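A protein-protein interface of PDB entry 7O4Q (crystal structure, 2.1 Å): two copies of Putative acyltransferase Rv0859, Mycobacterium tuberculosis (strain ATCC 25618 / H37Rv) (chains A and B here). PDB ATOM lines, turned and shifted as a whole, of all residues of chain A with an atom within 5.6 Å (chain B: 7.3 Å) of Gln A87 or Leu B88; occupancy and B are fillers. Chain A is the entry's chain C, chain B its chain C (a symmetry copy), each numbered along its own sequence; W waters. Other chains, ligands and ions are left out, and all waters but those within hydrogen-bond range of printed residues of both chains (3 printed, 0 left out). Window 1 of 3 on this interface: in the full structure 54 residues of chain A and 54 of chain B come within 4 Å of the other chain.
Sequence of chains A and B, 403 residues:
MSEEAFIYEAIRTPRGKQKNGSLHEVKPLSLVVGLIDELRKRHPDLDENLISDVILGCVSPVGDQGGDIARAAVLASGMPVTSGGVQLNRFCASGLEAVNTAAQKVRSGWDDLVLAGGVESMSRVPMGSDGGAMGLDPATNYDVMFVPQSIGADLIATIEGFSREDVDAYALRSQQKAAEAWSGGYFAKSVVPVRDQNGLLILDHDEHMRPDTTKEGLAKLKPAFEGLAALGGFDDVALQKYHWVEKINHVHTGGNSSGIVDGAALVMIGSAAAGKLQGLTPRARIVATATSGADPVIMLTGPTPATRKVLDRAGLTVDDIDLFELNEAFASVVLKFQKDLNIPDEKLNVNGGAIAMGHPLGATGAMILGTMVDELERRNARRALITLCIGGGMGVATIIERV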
ATOM      1  N   VAL A  54      12.092  -4.640  26.449  1.00  0.00           N
ATOM      2  CA  VAL A  54      12.256  -3.193  26.497  1.00  0.00           C
ATOM      3  C   VAL A  54      11.419  -2.608  25.366  1.00  0.00           C
ATOM      4  O   VAL A  54      11.669  -2.898  24.190  1.00  0.00           O
ATOM      5  CB  VAL A  54      13.731  -2.773  26.377  1.00  0.00           C
ATOM      6  CG1 VAL A  54      13.856  -1.258  26.339  1.00  0.00           C
ATOM      7  CG2 VAL A  54      14.529  -3.344  27.549  1.00  0.00           C
ATOM      8  N   LEU A  56       9.898   0.686  23.542  1.00  0.00           N
ATOM      9  CA  LEU A  56      10.093   2.118  23.344  1.00  0.00           C
ATOM     10  C   LEU A  56       9.124   2.646  22.296  1.00  0.00           C
ATOM     11  O   LEU A  56       9.050   2.111  21.184  1.00  0.00           O
ATOM     12  CB  LEU A  56      11.528   2.433  22.917  1.00  0.00           C
ATOM     13  CG  LEU A  56      12.629   2.154  23.940  1.00  0.00           C
ATOM     14  CD1 LEU A  56      13.980   2.625  23.417  1.00  0.00           C
ATOM     15  CD2 LEU A  56      12.293   2.825  25.265  1.00  0.00           C
ATOM     16  N   GLY A  57       8.391   3.699  22.651  1.00  0.00           N
ATOM     17  CA  GLY A  57       7.632   4.437  21.661  1.00  0.00           C
ATOM     18  C   GLY A  57       8.539   5.391  20.896  1.00  0.00           C
ATOM     19  O   GLY A  57       9.449   6.002  21.455  1.00  0.00           O
ATOM     20  N   CYS A  58       8.296   5.491  19.593  1.00  0.00           N
ATOM     21  CA  CYS A  58       9.064   6.394  18.741  1.00  0.00           C
ATOM     22  C   CYS A  58       8.221   6.722  17.521  1.00  0.00           C
ATOM     23  O   CYS A  58       7.845   5.818  16.768  1.00  0.00           O
ATOM     24  CB  CYS A  58      10.393   5.769  18.330  1.00  0.00           C
ATOM     25  SG  CYS A  58      11.469   6.918  17.461  1.00  0.00           S
ATOM     26  N   VAL A  59       7.937   8.007  17.319  1.00  0.00           N
ATOM     27  CA  VAL A  59       6.990   8.403  16.282  1.00  0.00           C
ATOM     28  C   VAL A  59       7.659   8.502  14.914  1.00  0.00           C
ATOM     29  O   VAL A  59       7.006   8.283  13.885  1.00  0.00           O
ATOM     30  CB  VAL A  59       6.313   9.720  16.689  1.00  0.00           C
ATOM     31  CG1 VAL A  59       5.285  10.155  15.648  1.00  0.00           C
ATOM     32  CG2 VAL A  59       5.659   9.551  18.044  1.00  0.00           C
ATOM     33  N   PRO A  61      10.550   6.607  13.521  1.00  0.00           N
ATOM     34  CA  PRO A  61      11.601   5.573  13.660  1.00  0.00           C
ATOM     35  C   PRO A  61      12.433   5.408  12.394  1.00  0.00           C
ATOM     36  O   PRO A  61      12.392   4.389  11.700  1.00  0.00           O
ATOM     37  CB  PRO A  61      10.782   4.324  13.994  1.00  0.00           C
ATOM     38  CG  PRO A  61       9.496   4.530  13.228  1.00  0.00           C
ATOM     39  CD  PRO A  61       9.221   6.016  13.275  1.00  0.00           C
ATOM     40  N   GLN A  65      16.870   6.891  14.624  1.00  0.00           N
ATOM     41  CA  GLN A  65      15.820   6.250  15.403  1.00  0.00           C
ATOM     42  C   GLN A  65      15.205   5.049  14.699  1.00  0.00           C
ATOM     43  O   GLN A  65      14.180   4.535  15.158  1.00  0.00           O
ATOM     44  CB  GLN A  65      14.732   7.268  15.749  1.00  0.00           C
ATOM     45  CG  GLN A  65      15.266   8.448  16.533  1.00  0.00           C
ATOM     46  CD  GLN A  65      14.201   9.465  16.873  1.00  0.00           C
ATOM     47  OE1 GLN A  65      14.362  10.246  17.806  1.00  0.00           O
ATOM     48  NE2 GLN A  65      13.110   9.470  16.112  1.00  0.00           N
ATOM     49  N   ASP A  68      14.724  -0.617  15.034  1.00  0.00           N
ATOM     50  CA  ASP A  68      14.393  -1.059  16.386  1.00  0.00           C
ATOM     51  C   ASP A  68      15.383  -0.492  17.396  1.00  0.00           C
ATOM     52  O   ASP A  68      16.274  -1.202  17.876  1.00  0.00           O
ATOM     53  CB  ASP A  68      14.358  -2.587  16.467  1.00  0.00           C
ATOM     54  CG  ASP A  68      13.715  -3.093  17.748  1.00  0.00           C
ATOM     55  OD1 ASP A  68      13.394  -2.268  18.627  1.00  0.00           O
ATOM     56  OD2 ASP A  68      13.516  -4.321  17.873  1.00  0.00           O
ATOM     57  N   ILE A  69      15.224   0.790  17.730  1.00  0.00           N
ATOM     58  CA  ILE A  69      16.178   1.443  18.617  1.00  0.00           C
ATOM     59  C   ILE A  69      16.145   0.806  20.002  1.00  0.00           C
ATOM     60  O   ILE A  69      17.145   0.838  20.733  1.00  0.00           O
ATOM     61  CB  ILE A  69      15.896   2.958  18.665  1.00  0.00           C
ATOM     62  CG1 ILE A  69      17.002   3.694  19.434  1.00  0.00           C
ATOM     63  CG2 ILE A  69      14.524   3.228  19.264  1.00  0.00           C
ATOM     64  CD1 ILE A  69      16.887   5.205  19.349  1.00  0.00           C
ATOM     65  N   ALA A  70      15.015   0.199  20.375  1.00  0.00           N
ATOM     66  CA  ALA A  70      14.911  -0.448  21.679  1.00  0.00           C
ATOM     67  C   ALA A  70      15.888  -1.613  21.798  1.00  0.00           C
ATOM     68  O   ALA A  70      16.522  -1.795  22.844  1.00  0.00           O
ATOM     69  CB  ALA A  70      13.477  -0.919  21.921  1.00  0.00           C
ATOM     70  N   GLY A  85      13.448  -6.049  23.182  1.00  0.00           N
ATOM     71  CA  GLY A  85      13.593  -4.781  22.492  1.00  0.00           C
ATOM     72  C   GLY A  85      12.633  -4.645  21.325  1.00  0.00           C
ATOM     73  O   GLY A  85      12.768  -5.351  20.320  1.00  0.00           O
ATOM     74  N   VAL A  86      11.655  -3.749  21.444  1.00  0.00           N
ATOM     75  CA  VAL A  86      10.639  -3.541  20.414  1.00  0.00           C
ATOM     76  C   VAL A  86      10.286  -2.060  20.361  1.00  0.00           C
ATOM     77  O   VAL A  86      10.187  -1.396  21.400  1.00  0.00           O
ATOM     78  CB  VAL A  86       9.384  -4.404  20.680  1.00  0.00           C
ATOM     79  CG1 VAL A  86       8.900  -4.219  22.108  1.00  0.00           C
ATOM     80  CG2 VAL A  86       8.271  -4.074  19.688  1.00  0.00           C
ATOM     81  N   GLN A  87      10.124  -1.535  19.148  1.00  0.00           N
ATOM     82  CA  GLN A  87       9.695  -0.159  18.929  1.00  0.00           C
ATOM     83  C   GLN A  87       8.229  -0.147  18.519  1.00  0.00           C
ATOM     84  O   GLN A  87       7.790  -1.005  17.752  1.00  0.00           O
ATOM     85  CB  GLN A  87      10.545   0.514  17.845  1.00  0.00           C
ATOM     86  CG  GLN A  87       9.998   1.856  17.329  1.00  0.00           C
ATOM     87  CD  GLN A  87       9.070   1.712  16.129  1.00  0.00           C
ATOM     88  OE1 GLN A  87       9.233   0.808  15.307  1.00  0.00           O
ATOM     89  NE2 GLN A  87       8.086   2.604  16.027  1.00  0.00           N
ATOM     90  N   LEU A  88       7.472   0.824  19.028  1.00  0.00           N
ATOM     91  CA  LEU A  88       6.089   0.991  18.609  1.00  0.00           C
ATOM     92  C   LEU A  88       5.811   2.456  18.296  1.00  0.00           C
ATOM     93  O   LEU A  88       6.504   3.359  18.770  1.00  0.00           O
ATOM     94  CB  LEU A  88       5.097   0.461  19.662  1.00  0.00           C
ATOM     95  CG  LEU A  88       5.082   0.953  21.111  1.00  0.00           C
ATOM     96  CD1 LEU A  88       4.413   2.317  21.250  1.00  0.00           C
ATOM     97  CD2 LEU A  88       4.369  -0.072  21.978  1.00  0.00           C
ATOM     98  N   ASN A  89       4.780   2.681  17.481  1.00  0.00           N
ATOM     99  CA  ASN A  89       4.375   4.031  17.094  1.00  0.00           C
ATOM    100  C   ASN A  89       2.853   4.118  17.138  1.00  0.00           C
ATOM    101  O   ASN A  89       2.167   3.578  16.263  1.00  0.00           O
ATOM    102  CB  ASN A  89       4.906   4.393  15.710  1.00  0.00           C
ATOM    103  CG  ASN A  89       4.363   5.724  15.201  1.00  0.00           C
ATOM    104  OD1 ASN A  89       4.003   6.602  15.981  1.00  0.00           O
ATOM    105  ND2 ASN A  89       4.305   5.873  13.882  1.00  0.00           N
ATOM    106  N   ILE B  55      -3.124  -3.866  15.535  1.00  0.00           N
ATOM    107  CA  ILE B  55      -1.697  -3.908  15.843  1.00  0.00           C
ATOM    108  C   ILE B  55      -0.982  -4.557  14.667  1.00  0.00           C
ATOM    109  O   ILE B  55      -1.150  -5.758  14.421  1.00  0.00           O
ATOM    110  CB  ILE B  55      -1.421  -4.680  17.141  1.00  0.00           C
ATOM    111  CG1 ILE B  55      -2.348  -4.201  18.261  1.00  0.00           C
ATOM    112  CG2 ILE B  55       0.039  -4.543  17.549  1.00  0.00           C
ATOM    113  CD1 ILE B  55      -2.218  -5.007  19.541  1.00  0.00           C
ATOM    114  N   LEU B  56      -0.168  -3.782  13.953  1.00  0.00           N
ATOM    115  CA  LEU B  56       0.532  -4.267  12.770  1.00  0.00           C
ATOM    116  C   LEU B  56       2.037  -4.227  12.991  1.00  0.00           C
ATOM    117  O   LEU B  56       2.589  -3.187  13.365  1.00  0.00           O
ATOM    118  CB  LEU B  56       0.176  -3.441  11.532  1.00  0.00           C
ATOM    119  CG  LEU B  56      -1.268  -3.524  11.039  1.00  0.00           C
ATOM    120  CD1 LEU B  56      -1.439  -2.747   9.740  1.00  0.00           C
ATOM    121  CD2 LEU B  56      -1.676  -4.982  10.859  1.00  0.00           C
ATOM    122  N   GLY B  57       2.695  -5.359  12.750  1.00  0.00           N
ATOM    123  CA  GLY B  57       4.144  -5.369  12.677  1.00  0.00           C
ATOM    124  C   GLY B  57       4.613  -4.868  11.319  1.00  0.00           C
ATOM    125  O   GLY B  57       4.011  -5.152  10.285  1.00  0.00           O
ATOM    126  N   CYS B  58       5.688  -4.087  11.338  1.00  0.00           N
ATOM    127  CA  CYS B  58       6.271  -3.562  10.107  1.00  0.00           C
ATOM    128  C   CYS B  58       7.730  -3.238  10.375  1.00  0.00           C
ATOM    129  O   CYS B  58       8.031  -2.414  11.245  1.00  0.00           O
ATOM    130  CB  CYS B  58       5.520  -2.324   9.624  1.00  0.00           C
ATOM    131  SG  CYS B  58       6.059  -1.765   8.002  1.00  0.00           S
ATOM    132  N   VAL B  59       8.631  -3.871   9.626  1.00  0.00           N
ATOM    133  CA  VAL B  59      10.054  -3.763   9.928  1.00  0.00           C
ATOM    134  C   VAL B  59      10.668  -2.506   9.319  1.00  0.00           C
ATOM    135  O   VAL B  59      11.633  -1.956   9.866  1.00  0.00           O
ATOM    136  CB  VAL B  59      10.770  -5.039   9.462  1.00  0.00           C
ATOM    137  CG1 VAL B  59      12.260  -4.985   9.790  1.00  0.00           C
ATOM    138  CG2 VAL B  59      10.125  -6.244  10.112  1.00  0.00           C
ATOM    139  N   SER B  60      10.126  -2.012   8.204  1.00  0.00           N
ATOM    140  CA  SER B  60      10.619  -0.800   7.551  1.00  0.00           C
ATOM    141  C   SER B  60       9.495   0.229   7.491  1.00  0.00           C
ATOM    142  O   SER B  60       8.954   0.513   6.413  1.00  0.00           O
ATOM    143  CB  SER B  60      11.152  -1.100   6.152  1.00  0.00           C
ATOM    144  OG  SER B  60      12.169  -2.085   6.197  1.00  0.00           O
ATOM    145  N   PRO B  61       9.126   0.817   8.629  1.00  0.00           N
ATOM    146  CA  PRO B  61       7.961   1.730   8.666  1.00  0.00           C
ATOM    147  C   PRO B  61       8.290   3.122   8.141  1.00  0.00           C
ATOM    148  O   PRO B  61       8.309   4.119   8.869  1.00  0.00           O
ATOM    149  CB  PRO B  61       7.599   1.730  10.153  1.00  0.00           C
ATOM    150  CG  PRO B  61       8.936   1.578  10.841  1.00  0.00           C
ATOM    151  CD  PRO B  61       9.756   0.668   9.955  1.00  0.00           C
ATOM    152  N   ASP B  68       2.374   5.314  11.094  1.00  0.00           N
ATOM    153  CA  ASP B  68       1.422   4.400  11.720  1.00  0.00           C
ATOM    154  C   ASP B  68       0.446   3.847  10.688  1.00  0.00           C
ATOM    155  O   ASP B  68      -0.712   4.275  10.620  1.00  0.00           O
ATOM    156  CB  ASP B  68       0.667   5.092  12.858  1.00  0.00           C
ATOM    157  CG  ASP B  68      -0.092   4.115  13.740  1.00  0.00           C
ATOM    158  OD1 ASP B  68      -0.128   2.912  13.413  1.00  0.00           O
ATOM    159  OD2 ASP B  68      -0.644   4.548  14.774  1.00  0.00           O
ATOM    160  N   ALA B  70      -1.067   1.166  10.613  1.00  0.00           N
ATOM    161  CA  ALA B  70      -2.209   0.497  11.230  1.00  0.00           C
ATOM    162  C   ALA B  70      -3.381   1.455  11.411  1.00  0.00           C
ATOM    163  O   ALA B  70      -4.536   1.086  11.170  1.00  0.00           O
ATOM    164  CB  ALA B  70      -1.799  -0.116  12.569  1.00  0.00           C
ATOM    165  N   VAL B  86      -1.791   0.795  15.844  1.00  0.00           N
ATOM    166  CA  VAL B  86      -0.423   0.960  16.330  1.00  0.00           C
ATOM    167  C   VAL B  86       0.506   0.088  15.494  1.00  0.00           C
ATOM    168  O   VAL B  86       0.161  -1.046  15.141  1.00  0.00           O
ATOM    169  CB  VAL B  86      -0.313   0.612  17.832  1.00  0.00           C
ATOM    170  CG1 VAL B  86      -0.938  -0.746  18.113  1.00  0.00           C
ATOM    171  CG2 VAL B  86       1.140   0.642  18.299  1.00  0.00           C
ATOM    172  N   GLN B  87       1.675   0.629  15.154  1.00  0.00           N
ATOM    173  CA  GLN B  87       2.711  -0.106  14.438  1.00  0.00           C
ATOM    174  C   GLN B  87       3.812  -0.504  15.411  1.00  0.00           C
ATOM    175  O   GLN B  87       4.178   0.277  16.290  1.00  0.00           O
ATOM    176  CB  GLN B  87       3.299   0.741  13.303  1.00  0.00           C
ATOM    177  CG  GLN B  87       4.587   0.183  12.675  1.00  0.00           C
ATOM    178  CD  GLN B  87       5.858   0.690  13.346  1.00  0.00           C
ATOM    179  OE1 GLN B  87       5.906   1.818  13.842  1.00  0.00           O
ATOM    180  NE2 GLN B  87       6.894  -0.147  13.368  1.00  0.00           N
ATOM    181  N   LEU B  88       4.340  -1.717  15.255  1.00  0.00           N
ATOM    182  CA  LEU B  88       5.474  -2.148  16.058  1.00  0.00           C
ATOM    183  C   LEU B  88       6.531  -2.788  15.168  1.00  0.00           C
ATOM    184  O   LEU B  88       6.246  -3.260  14.065  1.00  0.00           O
ATOM    185  CB  LEU B  88       5.053  -3.112  17.184  1.00  0.00           C
ATOM    186  CG  LEU B  88       4.299  -4.417  16.923  1.00  0.00           C
ATOM    187  CD1 LEU B  88       5.217  -5.519  16.400  1.00  0.00           C
ATOM    188  CD2 LEU B  88       3.618  -4.866  18.205  1.00  0.00           C
ATOM    189  N   ASN B  89       7.769  -2.795  15.665  1.00  0.00           N
ATOM    190  CA  ASN B  89       8.894  -3.383  14.941  1.00  0.00           C
ATOM    191  C   ASN B  89       9.750  -4.175  15.924  1.00  0.00           C
ATOM    192  O   ASN B  89      10.477  -3.591  16.736  1.00  0.00           O
ATOM    193  CB  ASN B  89       9.718  -2.312  14.233  1.00  0.00           C
ATOM    194  CG  ASN B  89      10.995  -2.867  13.610  1.00  0.00           C
ATOM    195  OD1 ASN B  89      11.073  -4.043  13.266  1.00  0.00           O
ATOM    196  ND2 ASN B  89      12.002  -2.012  13.466  1.00  0.00           N
ATOM    197  N   ARG B  90       9.656  -5.503  15.855  1.00  0.00           N
ATOM    198  CA  ARG B  90      10.663  -6.364  16.464  1.00  0.00           C
ATOM    199  C   ARG B  90      11.297  -7.207  15.367  1.00  0.00           C
ATOM    200  O   ARG B  90      11.375  -8.435  15.482  1.00  0.00           O
ATOM    201  CB  ARG B  90      10.069  -7.256  17.559  1.00  0.00           C
ATOM    202  CG  ARG B  90      11.128  -7.802  18.518  1.00  0.00           C
ATOM    203  CD  ARG B  90      10.670  -9.046  19.267  1.00  0.00           C
ATOM    204  NE  ARG B  90       9.614  -8.778  20.239  1.00  0.00           N
ATOM    205  CZ  ARG B  90       9.822  -8.292  21.459  1.00  0.00           C
ATOM    206  NH1 ARG B  90      11.053  -8.004  21.862  1.00  0.00           N
ATOM    207  NH2 ARG B  90       8.799  -8.086  22.278  1.00  0.00           N
ATOM    208  N   PHE B  91      11.728  -6.546  14.289  1.00  0.00           N
ATOM    209  CA  PHE B  91      12.347  -7.194  13.139  1.00  0.00           C
ATOM    210  C   PHE B  91      11.477  -8.328  12.603  1.00  0.00           C
ATOM    211  O   PHE B  91      10.248  -8.210  12.573  1.00  0.00           O
ATOM    212  CB  PHE B  91      13.742  -7.704  13.502  1.00  0.00           C
ATOM    213  CG  PHE B  91      14.711  -6.611  13.861  1.00  0.00           C
ATOM    214  CD1 PHE B  91      14.769  -5.444  13.115  1.00  0.00           C
ATOM    215  CD2 PHE B  91      15.557  -6.748  14.951  1.00  0.00           C
ATOM    216  CE1 PHE B  91      15.660  -4.435  13.442  1.00  0.00           C
ATOM    217  CE2 PHE B  91      16.452  -5.744  15.285  1.00  0.00           C
ATOM    218  CZ  PHE B  91      16.505  -4.587  14.529  1.00  0.00           C
ATOM    219  N   ALA B  93      10.235 -10.887  13.631  1.00  0.00           N
ATOM    220  CA  ALA B  93       9.187 -11.426  14.483  1.00  0.00           C
ATOM    221  C   ALA B  93       8.027 -10.465  14.687  1.00  0.00           C
ATOM    222  O   ALA B  93       7.137 -10.758  15.494  1.00  0.00           O
ATOM    223  CB  ALA B  93       9.765 -11.809  15.839  1.00  0.00           C
ATOM    224  N   SER B  94       8.011  -9.336  13.976  1.00  0.00           N
ATOM    225  CA  SER B  94       7.026  -8.295  14.255  1.00  0.00           C
ATOM    226  C   SER B  94       5.601  -8.813  14.105  1.00  0.00           C
ATOM    227  O   SER B  94       4.713  -8.436  14.879  1.00  0.00           O
ATOM    228  CB  SER B  94       7.264  -7.093  13.342  1.00  0.00           C
ATOM    229  OG  SER B  94       8.555  -6.545  13.556  1.00  0.00           O
ATOM    230  N   GLY B  95       5.362  -9.682  13.122  1.00  0.00           N
ATOM    231  CA  GLY B  95       4.012 -10.181  12.909  1.00  0.00           C
ATOM    232  C   GLY B  95       3.526 -11.062  14.044  1.00  0.00           C
ATOM    233  O   GLY B  95       2.358 -10.993  14.440  1.00  0.00           O
ATOM    234  N   LEU B  96       4.410 -11.906  14.580  1.00  0.00           N
ATOM    235  CA  LEU B  96       4.041 -12.716  15.735  1.00  0.00           C
ATOM    236  C   LEU B  96       3.997 -11.885  17.010  1.00  0.00           C
ATOM    237  O   LEU B  96       3.162 -12.144  17.883  1.00  0.00           O
ATOM    238  CB  LEU B  96       5.016 -13.887  15.902  1.00  0.00           C
ATOM    239  CG  LEU B  96       4.644 -14.896  16.995  1.00  0.00           C
ATOM    240  CD1 LEU B  96       3.296 -15.546  16.697  1.00  0.00           C
ATOM    241  CD2 LEU B  96       5.719 -15.954  17.163  1.00  0.00           C
ATOM    242  N   GLU B  97       4.879 -10.891  17.136  1.00  0.00           N
ATOM    243  CA  GLU B  97       4.836 -10.012  18.301  1.00  0.00           C
ATOM    244  C   GLU B  97       3.500  -9.289  18.391  1.00  0.00           C
ATOM    245  O   GLU B  97       2.928  -9.159  19.478  1.00  0.00           O
ATOM    246  CB  GLU B  97       5.987  -9.006  18.249  1.00  0.00           C
ATOM    247  CG  GLU B  97       5.990  -8.015  19.409  1.00  0.00           C
ATOM    248  CD  GLU B  97       6.057  -8.709  20.758  1.00  0.00           C
ATOM    249  OE1 GLU B  97       6.819  -9.692  20.885  1.00  0.00           O
ATOM    250  OE2 GLU B  97       5.340  -8.278  21.687  1.00  0.00           O
ATOM    251  N   ALA B  98       2.989  -8.812  17.256  1.00  0.00           N
ATOM    252  CA  ALA B  98       1.680  -8.168  17.247  1.00  0.00           C
ATOM    253  C   ALA B  98       0.598  -9.119  17.742  1.00  0.00           C
ATOM    254  O   ALA B  98      -0.279  -8.723  18.518  1.00  0.00           O
ATOM    255  CB  ALA B  98       1.354  -7.664  15.840  1.00  0.00           C
ATOM    256  N   VAL B  99       0.655 -10.383  17.313  1.00  0.00           N
ATOM    257  CA  VAL B  99      -0.318 -11.375  17.766  1.00  0.00           C
ATOM    258  C   VAL B  99      -0.183 -11.608  19.267  1.00  0.00           C
ATOM    259  O   VAL B  99      -1.178 -11.632  20.001  1.00  0.00           O
ATOM    260  CB  VAL B  99      -0.156 -12.686  16.974  1.00  0.00           C
ATOM    261  CG1 VAL B  99      -0.888 -13.828  17.670  1.00  0.00           C
ATOM    262  CG2 VAL B  99      -0.658 -12.512  15.542  1.00  0.00           C
ATOM    263  N   THR B 101       1.154  -9.581  21.518  1.00  0.00           N
ATOM    264  CA  THR B 101       0.722  -8.369  22.206  1.00  0.00           C
ATOM    265  C   THR B 101      -0.798  -8.267  22.236  1.00  0.00           C
ATOM    266  O   THR B 101      -1.380  -7.863  23.251  1.00  0.00           O
ATOM    267  CB  THR B 101       1.338  -7.142  21.532  1.00  0.00           C
ATOM    268  OG1 THR B 101       2.760  -7.174  21.705  1.00  0.00           O
ATOM    269  CG2 THR B 101       0.785  -5.854  22.134  1.00  0.00           C
ATOM    270  N   ALA B 102      -1.460  -8.654  21.144  1.00  0.00           N
ATOM    271  CA  ALA B 102      -2.918  -8.664  21.132  1.00  0.00           C
ATOM    272  C   ALA B 102      -3.468  -9.660  22.145  1.00  0.00           C
ATOM    273  O   ALA B 102      -4.438  -9.363  22.855  1.00  0.00           O
ATOM    274  CB  ALA B 102      -3.430  -8.986  19.728  1.00  0.00           C
ATOM    275  N   GLY B 117      -1.550  -8.328  13.133  1.00  0.00           N
ATOM    276  CA  GLY B 117      -0.962  -8.842  11.904  1.00  0.00           C
ATOM    277  C   GLY B 117       0.291  -8.083  11.530  1.00  0.00           C
ATOM    278  O   GLY B 117       1.031  -7.603  12.397  1.00  0.00           O
ATOM    279  N   ASP B 130      14.780   2.105   6.622  1.00  0.00           N
ATOM    280  CA  ASP B 130      14.609   2.901   7.830  1.00  0.00           C
ATOM    281  C   ASP B 130      15.923   3.223   8.532  1.00  0.00           C
ATOM    282  O   ASP B 130      15.916   4.004   9.492  1.00  0.00           O
ATOM    283  CB  ASP B 130      13.677   2.178   8.810  1.00  0.00           C
ATOM    284  CG  ASP B 130      14.149   0.769   9.142  1.00  0.00           C
ATOM    285  OD1 ASP B 130      14.590   0.045   8.219  1.00  0.00           O
ATOM    286  OD2 ASP B 130      14.077   0.386  10.331  1.00  0.00           O
ATOM    287  N   GLY B 362       7.644  -7.928   8.218  1.00  0.00           N
ATOM    288  CA  GLY B 362       6.671  -7.596   9.248  1.00  0.00           C
ATOM    289  C   GLY B 362       5.417  -8.452   9.246  1.00  0.00           C
ATOM    290  O   GLY B 362       4.677  -8.452  10.237  1.00  0.00           O
HETATM  291  O   HOH W   1       5.159   3.973  12.207  1.00  0.00           O
HETATM  292  O   HOH W   2      12.185   1.648  11.900  1.00  0.00           O
HETATM  293  O   HOH W   3      11.783   0.560  14.161  1.00  0.00           O
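The side-chain amide nitrogen (ND2) of Asn B89 sits close to the backbone NH (N) of Asp A68 (3.4 Å). The side-chain amide nitrogen of Gln B87 is in hydrogen-bond range of the side-chain amide oxygen of Gln A87, at 3.2 Å. The backbone carbonyl oxygen (O) of Gln A87 sits at hydrogen-bond distance from the backbone NH (N) of Asn B89 (2.7 Å). The backbone NH (N) of Asp B68 sits close to the side-chain amide nitrogen (ND2) of Asn A89 (3.4 Å). The backbone carbonyl oxygen of Gln B87 lies within hydrogen-bond range of the backbone NH of Asn A89, 2.7 Å away. N of Gly A85 sits close to NH1 of Arg B90.
The backbone carbonyl oxygen (O) of Val A86 is in hydrogen-bond range of the backbone NH (N) of Leu A56. The side-chain carboxylate (OD1) of Asp A68 lies within hydrogen-bond range of the backbone NH (N) of Gln A87, at 3.4 Å. N of Gln B87 lies within hydrogen-bond range of OD1 of Asp B68 (3.4 Å). The backbone NH (N) of Phe B91 is in hydrogen-bond range of the side-chain amide oxygen (OD1) of Asn B89 (2.8 Å). N of Arg B90 is in hydrogen-bond range of OG of Ser B94 (2.8 Å).
Among the printed residues, pairs that only touch across the chains: Pro A61 with Pro B61 (3.8 Å), Pro A61 with Asp B130 (3.9 Å), Asp A68 with Arg B90 (3.8 Å), Asp A68 with Phe B91 (3.5 Å), Val A86 with Asn B89 (3.7 Å), Val A86 with Arg B90 (3.9 Å), Gln A87 with Leu B88 (3.1 Å), Leu A88 with Gln B87 (3.1 Å) and Asn A89 with Val B86 (3.7 Å).
Of the printed residues of chain B, Gln A87 touches Gln B87 (3.2 Å), Leu B88 (3.1 Å) and Asn B89 (2.7 Å). Of chain A, only Gln A87 (3.1 Å) comes within 4 Å of Leu B88. Of the printed residues of chain A, Pro B61 touches Pro A61 (3.8 Å). Of the printed residues of chain A, Asn B89 touches Asp A68 (3.3 Å), Val A86 (3.7 Å) and Gln A87 (2.7 Å). Printed residues of chain A within 4 Å of Gln B87: Gln A87 (3.2 Å), Leu A88 (3.1 Å) and Asn A89 (2.7 Å). Gln A65 touches none of the printed residues of chain B. Ile B55 touches none of the printed residues of chain A. The nearest residue of chain A that does not touch Leu B88 is Leu A88 (4.1 Å). The nearest printed residue of chain B that does not touch Asp A68 is Asp B130 (4.9 Å).
Hydrophobic or aromatic side chains of chain B within 4 Å of the printed part of chain A: Pro B61, Val B86, Leu B88 and Phe B91. Printed residues of chain A that touch a printed residue of chain B: Pro A61, Asp A68, Gly A85, Val A86, Gln A87, Leu A88 and Asn A89. Among the printed residues, 15 pairs touch across the chains. Among the printed residues, no Asp or Glu carboxylate lies within 4 Å of a Lys or Arg side-chain nitrogen of the other chain.
Pro A61 touches its own counterpart, Pro B61. Asp A68 touches Asn B89, and with the chains exchanged Asn A89 touches Asp B68. Val A86 touches Asn B89, and with the chains exchanged Asn A89 touches Val B86. Positions printed for both chains: 56, 57, 58, 59, 61, 68, 70, 86, 87, 88 and 89. Of the 15 pairs that touch across the chains among the printed residues, 10 have their exchanged pair printed and touching as well.
Water W1 lies within hydrogen-bond range of ND2 of Asn A89, OE1 of Gln B87 and N of Asp B68. Water W3 lies within hydrogen-bond range of ND2 of Asn B89 (2.7 Å), OE1 of Gln A87 (2.8 Å) and N of Asp A68 (3.3 Å). Water W2 lies within hydrogen-bond range of the backbone carbonyl oxygen (O) of Pro A61 (2.8 Å) and the side-chain carboxylate (OD2) of Asp B130 (2.8 Å).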
